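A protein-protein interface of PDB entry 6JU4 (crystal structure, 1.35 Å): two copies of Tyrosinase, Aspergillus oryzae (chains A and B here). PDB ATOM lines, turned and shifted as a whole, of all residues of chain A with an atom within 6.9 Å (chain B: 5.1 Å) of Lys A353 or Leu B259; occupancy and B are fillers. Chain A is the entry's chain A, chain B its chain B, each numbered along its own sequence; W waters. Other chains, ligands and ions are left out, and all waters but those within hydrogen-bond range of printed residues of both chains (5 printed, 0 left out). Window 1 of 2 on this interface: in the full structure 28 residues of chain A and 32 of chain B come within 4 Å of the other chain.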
ATOM      1  N   TYR A 240      32.839   9.137 -11.283  1.00  0.00           N
ATOM      2  CA  TYR A 240      32.093  10.347 -10.937  1.00  0.00           C
ATOM      3  C   TYR A 240      32.324  10.813  -9.512  1.00  0.00           C
ATOM      4  O   TYR A 240      31.536  11.626  -8.995  1.00  0.00           O
ATOM      5  CB  TYR A 240      30.574  10.198 -11.176  1.00  0.00           C
ATOM      6  CG  TYR A 240      30.244  10.111 -12.660  1.00  0.00           C
ATOM      7  CD1 TYR A 240      30.270   8.876 -13.308  1.00  0.00           C
ATOM      8  CD2 TYR A 240      29.910  11.238 -13.413  1.00  0.00           C
ATOM      9  CE1 TYR A 240      29.993   8.768 -14.651  1.00  0.00           C
ATOM     10  CE2 TYR A 240      29.609  11.139 -14.769  1.00  0.00           C
ATOM     11  CZ  TYR A 240      29.652   9.894 -15.367  1.00  0.00           C
ATOM     12  OH  TYR A 240      29.357   9.767 -16.705  1.00  0.00           O
ATOM     13  N   LEU A 243      34.568  15.696  -7.073  1.00  0.00           N
ATOM     14  CA  LEU A 243      33.833  16.943  -7.221  1.00  0.00           C
ATOM     15  C   LEU A 243      34.523  18.034  -6.392  1.00  0.00           C
ATOM     16  O   LEU A 243      34.985  17.784  -5.271  1.00  0.00           O
ATOM     17  CB  LEU A 243      32.375  16.853  -6.761  1.00  0.00           C
ATOM     18  CG  LEU A 243      31.390  16.082  -7.654  1.00  0.00           C
ATOM     19  CD1 LEU A 243      31.526  14.593  -7.419  1.00  0.00           C
ATOM     20  CD2 LEU A 243      29.967  16.547  -7.358  1.00  0.00           C
ATOM     21  N   GLU A 244      34.559  19.226  -6.960  1.00  0.00           N
ATOM     22  CA  GLU A 244      35.105  20.408  -6.274  1.00  0.00           C
ATOM     23  C   GLU A 244      34.213  20.747  -5.086  1.00  0.00           C
ATOM     24  O   GLU A 244      33.008  20.469  -5.073  1.00  0.00           O
ATOM     25  CB  GLU A 244      35.182  21.584  -7.245  1.00  0.00           C
ATOM     26  CG  GLU A 244      35.907  22.832  -6.779  1.00  0.00           C
ATOM     27  CD  GLU A 244      36.097  23.806  -7.930  1.00  0.00           C
ATOM     28  OE1 GLU A 244      35.150  24.565  -8.253  1.00  0.00           O
ATOM     29  OE2 GLU A 244      37.202  23.826  -8.523  1.00  0.00           O
ATOM     30  N   TYR A 246      34.165  19.655  -2.002  1.00  0.00           N
ATOM     31  CA  TYR A 246      34.132  18.681  -0.909  1.00  0.00           C
ATOM     32  C   TYR A 246      35.529  18.593  -0.314  1.00  0.00           C
ATOM     33  O   TYR A 246      36.512  18.970  -0.968  1.00  0.00           O
ATOM     34  CB  TYR A 246      33.627  17.304  -1.404  1.00  0.00           C
ATOM     35  CG  TYR A 246      32.217  17.518  -1.917  1.00  0.00           C
ATOM     36  CD1 TYR A 246      31.120  17.445  -1.072  1.00  0.00           C
ATOM     37  CD2 TYR A 246      32.010  17.849  -3.250  1.00  0.00           C
ATOM     38  CE1 TYR A 246      29.840  17.663  -1.561  1.00  0.00           C
ATOM     39  CE2 TYR A 246      30.740  18.081  -3.731  1.00  0.00           C
ATOM     40  CZ  TYR A 246      29.657  17.986  -2.885  1.00  0.00           C
ATOM     41  OH  TYR A 246      28.412  18.235  -3.413  1.00  0.00           O
ATOM     42  N   ASN A 257      30.051   5.561  -8.615  1.00  0.00           N
ATOM     43  CA  ASN A 257      28.668   5.989  -8.832  1.00  0.00           C
ATOM     44  C   ASN A 257      28.187   5.334 -10.122  1.00  0.00           C
ATOM     45  O   ASN A 257      28.087   5.948 -11.176  1.00  0.00           O
ATOM     46  CB  ASN A 257      28.580   7.516  -8.879  1.00  0.00           C
ATOM     47  CG  ASN A 257      27.145   7.998  -8.746  1.00  0.00           C
ATOM     48  OD1 ASN A 257      26.200   7.221  -8.947  1.00  0.00           O
ATOM     49  ND2 ASN A 257      26.988   9.277  -8.413  1.00  0.00           N
ATOM     50  N   ARG A 260      25.073   6.686 -11.928  1.00  0.00           N
ATOM     51  CA  ARG A 260      25.348   7.878 -12.718  1.00  0.00           C
ATOM     52  C   ARG A 260      26.058   7.489 -14.006  1.00  0.00           C
ATOM     53  O   ARG A 260      25.722   8.048 -15.056  1.00  0.00           O
ATOM     54  CB  ARG A 260      26.196   8.880 -11.932  1.00  0.00           C
ATOM     55  CG  ARG A 260      26.629  10.098 -12.751  1.00  0.00           C
ATOM     56  CD  ARG A 260      25.427  10.923 -13.162  1.00  0.00           C
ATOM     57  NE  ARG A 260      25.706  12.070 -14.014  1.00  0.00           N
ATOM     58  CZ  ARG A 260      25.608  12.012 -15.343  1.00  0.00           C
ATOM     59  NH1 ARG A 260      25.292  10.886 -15.964  1.00  0.00           N
ATOM     60  NH2 ARG A 260      25.851  13.111 -16.039  1.00  0.00           N
ATOM     61  N   ARG A 346      30.925  22.595 -11.704  1.00  0.00           N
ATOM     62  CA  ARG A 346      29.974  23.283 -12.557  1.00  0.00           C
ATOM     63  C   ARG A 346      29.760  24.684 -11.996  1.00  0.00           C
ATOM     64  O   ARG A 346      29.674  24.817 -10.772  1.00  0.00           O
ATOM     65  CB  ARG A 346      28.632  22.559 -12.625  1.00  0.00           C
ATOM     66  CG  ARG A 346      27.690  23.123 -13.684  1.00  0.00           C
ATOM     67  CD  ARG A 346      26.516  22.164 -13.903  1.00  0.00           C
ATOM     68  NE  ARG A 346      26.996  20.944 -14.547  1.00  0.00           N
ATOM     69  CZ  ARG A 346      26.254  19.948 -15.016  1.00  0.00           C
ATOM     70  NH1 ARG A 346      24.921  19.956 -14.948  1.00  0.00           N
ATOM     71  NH2 ARG A 346      26.836  18.895 -15.578  1.00  0.00           N
ATOM     72  N   ARG A 349      24.522  27.773  -9.361  1.00  0.00           N
ATOM     73  CA  ARG A 349      23.780  27.131  -8.289  1.00  0.00           C
ATOM     74  C   ARG A 349      23.052  25.903  -8.824  1.00  0.00           C
ATOM     75  O   ARG A 349      22.268  26.023  -9.760  1.00  0.00           O
ATOM     76  CB  ARG A 349      22.758  28.102  -7.688  1.00  0.00           C
ATOM     77  CG  ARG A 349      21.609  27.384  -6.992  1.00  0.00           C
ATOM     78  CD  ARG A 349      20.563  28.369  -6.503  1.00  0.00           C
ATOM     79  NE  ARG A 349      19.531  28.644  -7.494  1.00  0.00           N
ATOM     80  CZ  ARG A 349      18.308  29.082  -7.218  1.00  0.00           C
ATOM     81  NH1 ARG A 349      17.923  29.305  -5.967  1.00  0.00           N
ATOM     82  NH2 ARG A 349      17.457  29.295  -8.217  1.00  0.00           N
ATOM     83  N   HIS A 350      23.356  24.764  -8.224  1.00  0.00           N
ATOM     84  CA  HIS A 350      22.675  23.513  -8.560  1.00  0.00           C
ATOM     85  C   HIS A 350      22.466  22.628  -7.345  1.00  0.00           C
ATOM     86  O   HIS A 350      23.433  22.183  -6.722  1.00  0.00           O
ATOM     87  CB  HIS A 350      23.456  22.715  -9.617  1.00  0.00           C
ATOM     88  CG  HIS A 350      23.754  23.544 -10.822  1.00  0.00           C
ATOM     89  ND1 HIS A 350      22.893  23.636 -11.888  1.00  0.00           N
ATOM     90  CD2 HIS A 350      24.809  24.342 -11.104  1.00  0.00           C
ATOM     91  CE1 HIS A 350      23.415  24.448 -12.787  1.00  0.00           C
ATOM     92  NE2 HIS A 350      24.574  24.897 -12.338  1.00  0.00           N
ATOM     93  N   ASP A 351      21.216  22.313  -7.015  1.00  0.00           N
ATOM     94  CA  ASP A 351      21.015  21.329  -5.951  1.00  0.00           C
ATOM     95  C   ASP A 351      21.297  19.911  -6.432  1.00  0.00           C
ATOM     96  O   ASP A 351      22.002  19.196  -5.730  1.00  0.00           O
ATOM     97  CB  ASP A 351      19.584  21.420  -5.429  1.00  0.00           C
ATOM     98  CG  ASP A 351      19.357  22.757  -4.739  1.00  0.00           C
ATOM     99  OD1 ASP A 351      20.304  23.316  -4.133  1.00  0.00           O
ATOM    100  OD2 ASP A 351      18.210  23.224  -4.850  1.00  0.00           O
ATOM    101  N   LEU A 352      20.769  19.536  -7.594  1.00  0.00           N
ATOM    102  CA  LEU A 352      21.082  18.252  -8.210  1.00  0.00           C
ATOM    103  C   LEU A 352      22.439  18.332  -8.906  1.00  0.00           C
ATOM    104  O   LEU A 352      22.606  19.156  -9.806  1.00  0.00           O
ATOM    105  CB  LEU A 352      19.988  17.839  -9.201  1.00  0.00           C
ATOM    106  CG  LEU A 352      20.285  16.571 -10.018  1.00  0.00           C
ATOM    107  CD1 LEU A 352      20.414  15.351  -9.116  1.00  0.00           C
ATOM    108  CD2 LEU A 352      19.222  16.369 -11.093  1.00  0.00           C
ATOM    109  N   LYS A 353      23.371  17.492  -8.455  1.00  0.00           N
ATOM    110  CA  LYS A 353      24.751  17.576  -8.938  1.00  0.00           C
ATOM    111  C   LYS A 353      25.054  16.385  -9.827  1.00  0.00           C
ATOM    112  O   LYS A 353      25.271  15.273  -9.355  1.00  0.00           O
ATOM    113  CB  LYS A 353      25.725  17.705  -7.759  1.00  0.00           C
ATOM    114  CG  LYS A 353      25.413  18.955  -6.934  1.00  0.00           C
ATOM    115  CD  LYS A 353      26.347  19.147  -5.766  1.00  0.00           C
ATOM    116  CE  LYS A 353      25.699  19.920  -4.630  1.00  0.00           C
ATOM    117  NZ  LYS A 353      25.296  21.295  -5.022  1.00  0.00           N
ATOM    118  N   LEU A 354      25.016  16.659 -11.124  1.00  0.00           N
ATOM    119  CA  LEU A 354      25.146  15.605 -12.129  1.00  0.00           C
ATOM    120  C   LEU A 354      26.578  15.462 -12.617  1.00  0.00           C
ATOM    121  O   LEU A 354      26.912  14.581 -13.415  1.00  0.00           O
ATOM    122  CB  LEU A 354      24.182  15.873 -13.291  1.00  0.00           C
ATOM    123  CG  LEU A 354      22.701  15.686 -12.958  1.00  0.00           C
ATOM    124  CD1 LEU A 354      21.803  16.393 -13.953  1.00  0.00           C
ATOM    125  CD2 LEU A 354      22.355  14.205 -12.899  1.00  0.00           C
ATOM    126  N   TRP A 355      27.470  16.336 -12.147  1.00  0.00           N
ATOM    127  CA  TRP A 355      28.861  16.244 -12.589  1.00  0.00           C
ATOM    128  C   TRP A 355      29.655  15.351 -11.648  1.00  0.00           C
ATOM    129  O   TRP A 355      29.086  14.614 -10.851  1.00  0.00           O
ATOM    130  CB  TRP A 355      29.498  17.618 -12.720  1.00  0.00           C
ATOM    131  CG  TRP A 355      29.542  18.439 -11.462  1.00  0.00           C
ATOM    132  CD1 TRP A 355      30.589  18.570 -10.597  1.00  0.00           C
ATOM    133  CD2 TRP A 355      28.489  19.263 -10.942  1.00  0.00           C
ATOM    134  NE1 TRP A 355      30.241  19.411  -9.560  1.00  0.00           N
ATOM    135  CE2 TRP A 355      28.961  19.853  -9.757  1.00  0.00           C
ATOM    136  CE3 TRP A 355      27.185  19.556 -11.359  1.00  0.00           C
ATOM    137  CZ2 TRP A 355      28.193  20.722  -8.978  1.00  0.00           C
ATOM    138  CZ3 TRP A 355      26.429  20.418 -10.584  1.00  0.00           C
ATOM    139  CH2 TRP A 355      26.924  20.992  -9.413  1.00  0.00           C
ATOM    140  N   GLY A 356      30.978  15.353 -11.789  1.00  0.00           N
ATOM    141  CA  GLY A 356      31.824  14.428 -11.042  1.00  0.00           C
ATOM    142  C   GLY A 356      32.793  13.749 -11.994  1.00  0.00           C
ATOM    143  O   GLY A 356      32.434  13.344 -13.097  1.00  0.00           O
ATOM    144  N   GLU B 167      24.982  24.584   1.893  1.00  0.00           N
ATOM    145  CA  GLU B 167      24.038  23.472   1.809  1.00  0.00           C
ATOM    146  C   GLU B 167      24.243  22.570   3.022  1.00  0.00           C
ATOM    147  O   GLU B 167      25.311  22.589   3.639  1.00  0.00           O
ATOM    148  CB  GLU B 167      24.143  22.704   0.496  1.00  0.00           C
ATOM    149  CG  GLU B 167      25.314  21.769   0.364  1.00  0.00           C
ATOM    150  CD  GLU B 167      25.361  20.912  -0.883  1.00  0.00           C
ATOM    151  OE1 GLU B 167      26.316  20.114  -1.019  1.00  0.00           O
ATOM    152  OE2 GLU B 167      24.454  21.009  -1.740  1.00  0.00           O
ATOM    153  N   ASN B 257      25.211   6.251  -1.443  1.00  0.00           N
ATOM    154  CA  ASN B 257      25.000   7.334  -2.407  1.00  0.00           C
ATOM    155  C   ASN B 257      24.822   8.631  -1.625  1.00  0.00           C
ATOM    156  O   ASN B 257      23.727   9.155  -1.500  1.00  0.00           O
ATOM    157  CB  ASN B 257      23.835   7.049  -3.358  1.00  0.00           C
ATOM    158  CG  ASN B 257      23.841   7.944  -4.588  1.00  0.00           C
ATOM    159  OD1 ASN B 257      24.460   9.016  -4.606  1.00  0.00           O
ATOM    160  ND2 ASN B 257      23.117   7.490  -5.608  1.00  0.00           N
ATOM    161  N   TRP B 258      25.941   9.125  -1.097  1.00  0.00           N
ATOM    162  CA  TRP B 258      25.923  10.242  -0.164  1.00  0.00           C
ATOM    163  C   TRP B 258      25.543  11.529  -0.896  1.00  0.00           C
ATOM    164  O   TRP B 258      24.929  12.425  -0.308  1.00  0.00           O
ATOM    165  CB  TRP B 258      27.239  10.366   0.613  1.00  0.00           C
ATOM    166  CG  TRP B 258      28.471  10.594  -0.208  1.00  0.00           C
ATOM    167  CD1 TRP B 258      29.384   9.674  -0.648  1.00  0.00           C
ATOM    168  CD2 TRP B 258      28.924  11.869  -0.691  1.00  0.00           C
ATOM    169  NE1 TRP B 258      30.380  10.304  -1.375  1.00  0.00           N
ATOM    170  CE2 TRP B 258      30.110  11.650  -1.414  1.00  0.00           C
ATOM    171  CE3 TRP B 258      28.428  13.175  -0.574  1.00  0.00           C
ATOM    172  CZ2 TRP B 258      30.788  12.710  -2.009  1.00  0.00           C
ATOM    173  CZ3 TRP B 258      29.109  14.223  -1.168  1.00  0.00           C
ATOM    174  CH2 TRP B 258      30.283  13.980  -1.881  1.00  0.00           C
ATOM    175  N   LEU B 259      25.868  11.591  -2.194  1.00  0.00           N
ATOM    176  CA  LEU B 259      25.452  12.764  -2.963  1.00  0.00           C
ATOM    177  C   LEU B 259      23.928  12.841  -3.056  1.00  0.00           C
ATOM    178  O   LEU B 259      23.322  13.917  -2.933  1.00  0.00           O
ATOM    179  CB  LEU B 259      26.062  12.729  -4.360  1.00  0.00           C
ATOM    180  CG  LEU B 259      26.399  14.023  -5.063  1.00  0.00           C
ATOM    181  CD1 LEU B 259      27.221  14.981  -4.219  1.00  0.00           C
ATOM    182  CD2 LEU B 259      27.136  13.674  -6.357  1.00  0.00           C
ATOM    183  N   ARG B 260      23.317  11.678  -3.278  1.00  0.00           N
ATOM    184  CA  ARG B 260      21.850  11.623  -3.350  1.00  0.00           C
ATOM    185  C   ARG B 260      21.194  11.932  -2.007  1.00  0.00           C
ATOM    186  O   ARG B 260      20.183  12.665  -1.924  1.00  0.00           O
ATOM    187  CB  ARG B 260      21.417  10.259  -3.888  1.00  0.00           C
ATOM    188  CG  ARG B 260      19.897  10.109  -3.860  1.00  0.00           C
ATOM    189  CD  ARG B 260      19.268  10.987  -4.916  1.00  0.00           C
ATOM    190  NE  ARG B 260      17.814  10.938  -4.952  1.00  0.00           N
ATOM    191  CZ  ARG B 260      17.015  11.720  -4.246  1.00  0.00           C
ATOM    192  NH1 ARG B 260      17.541  12.611  -3.412  1.00  0.00           N
ATOM    193  NH2 ARG B 260      15.698  11.622  -4.370  1.00  0.00           N
ATOM    194  N   ALA B 261      21.795  11.447  -0.927  1.00  0.00           N
ATOM    195  CA  ALA B 261      21.298  11.764   0.410  1.00  0.00           C
ATOM    196  C   ALA B 261      21.424  13.250   0.676  1.00  0.00           C
ATOM    197  O   ALA B 261      20.500  13.855   1.210  1.00  0.00           O
ATOM    198  CB  ALA B 261      22.025  10.932   1.457  1.00  0.00           C
ATOM    199  N   ASN B 262      22.535  13.878   0.277  1.00  0.00           N
ATOM    200  CA  ASN B 262      22.700  15.318   0.459  1.00  0.00           C
ATOM    201  C   ASN B 262      21.612  16.060  -0.313  1.00  0.00           C
ATOM    202  O   ASN B 262      21.042  17.044   0.200  1.00  0.00           O
ATOM    203  CB  ASN B 262      24.065  15.823   0.008  1.00  0.00           C
ATOM    204  CG  ASN B 262      25.179  15.510   0.987  1.00  0.00           C
ATOM    205  OD1 ASN B 262      24.939  14.937   2.056  1.00  0.00           O
ATOM    206  ND2 ASN B 262      26.412  15.842   0.622  1.00  0.00           N
ATOM    207  N   LEU B 263      21.291  15.597  -1.513  1.00  0.00           N
ATOM    208  CA  LEU B 263      20.233  16.265  -2.282  1.00  0.00           C
ATOM    209  C   LEU B 263      18.930  16.214  -1.507  1.00  0.00           C
ATOM    210  O   LEU B 263      18.227  17.224  -1.401  1.00  0.00           O
ATOM    211  CB  LEU B 263      20.090  15.588  -3.652  1.00  0.00           C
ATOM    212  CG  LEU B 263      18.937  16.092  -4.536  1.00  0.00           C
ATOM    213  CD1 LEU B 263      19.108  17.576  -4.829  1.00  0.00           C
ATOM    214  CD2 LEU B 263      18.855  15.286  -5.825  1.00  0.00           C
HETATM  215  O   HOH W   1      23.538   8.332  -8.642  1.00  0.00           O
HETATM  216  O   HOH W   2      24.315  10.609  -6.943  1.00  0.00           O
HETATM  217  O   HOH W   3      26.287  17.502  -1.950  1.00  0.00           O
HETATM  218  O   HOH W   4      22.614  18.708  -2.710  1.00  0.00           O
HETATM  219  O   HOH W   5      26.630   7.069  -5.706  1.00  0.00           O
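Positions printed for both chains: 257 and 260. Of the 7 pairs that touch across the chains among the printed residues, none has its exchanged pair printed and touching as well.
Hydrophobic or aromatic side chains of chain B within 4 Å of the printed part of chain A: Trp B258, Leu B259 and Leu B263.
Water W3 lies within hydrogen-bond range of the side-chain hydroxyl (OH) of Tyr A246, the side-chain carboxylate (OE1) of Glu B167 and the side-chain amide nitrogen (ND2) of Asn B262. Water W2 bridges the side-chain amide oxygen (OD1) of Asn B257 and the side-chain amide nitrogen (ND2) of Asn A257. Water W1 lies within hydrogen-bond range of the side-chain amide oxygen (OD1) of Asn A257 (2.9 Å) and the side-chain amide nitrogen (ND2) of Asn B257 (3.2 Å). Water W4 bridges OE2 of Glu B167 and O of Asp A351. Water W5 bridges OD1 of Asn B257 (3.1 Å) and OD1 of Asn A257 (3.3 Å).
Glu A244 touches none of the printed residues of chain B. Printed residues of chain B within 4 Å of Asp A351: Leu B263. Printed residues of chain B within 4 Å of Leu A352: Leu B263. Lys A353 touches just these residues of chain B: Glu B167 (3.3 Å) and Leu B259 (3.9 Å). Of the printed residues of chain A, Trp B258 touches Tyr A246. The nearest printed residue of chain B that does not touch Lys A353 is Leu B263 (5.6 Å).
Glu B167 touches Tyr A246. Trp B258 touches Tyr A246. OH of Tyr A246 touches CD1 of Leu B259, 3.6 Å away. Leu B263 touches Asp A351 (CD1 to O, 3.4 Å). Leu A352 touches Leu B263 (CD1 to CD2, 3.6 Å). O of Lys A353 touches CD2 of Leu B259, 3.9 Å away.
The side-chain carboxylate of Glu B167 lies within salt-bridge range of the side-chain amino group of Lys A353.
The backbone carbonyl oxygen of His A350 is in hydrogen-bond range of the side-chain amino group of Lys A353 (2.7 Å). O of Trp B258 lies close to OD1 of Asn B262 (3.4 Å).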
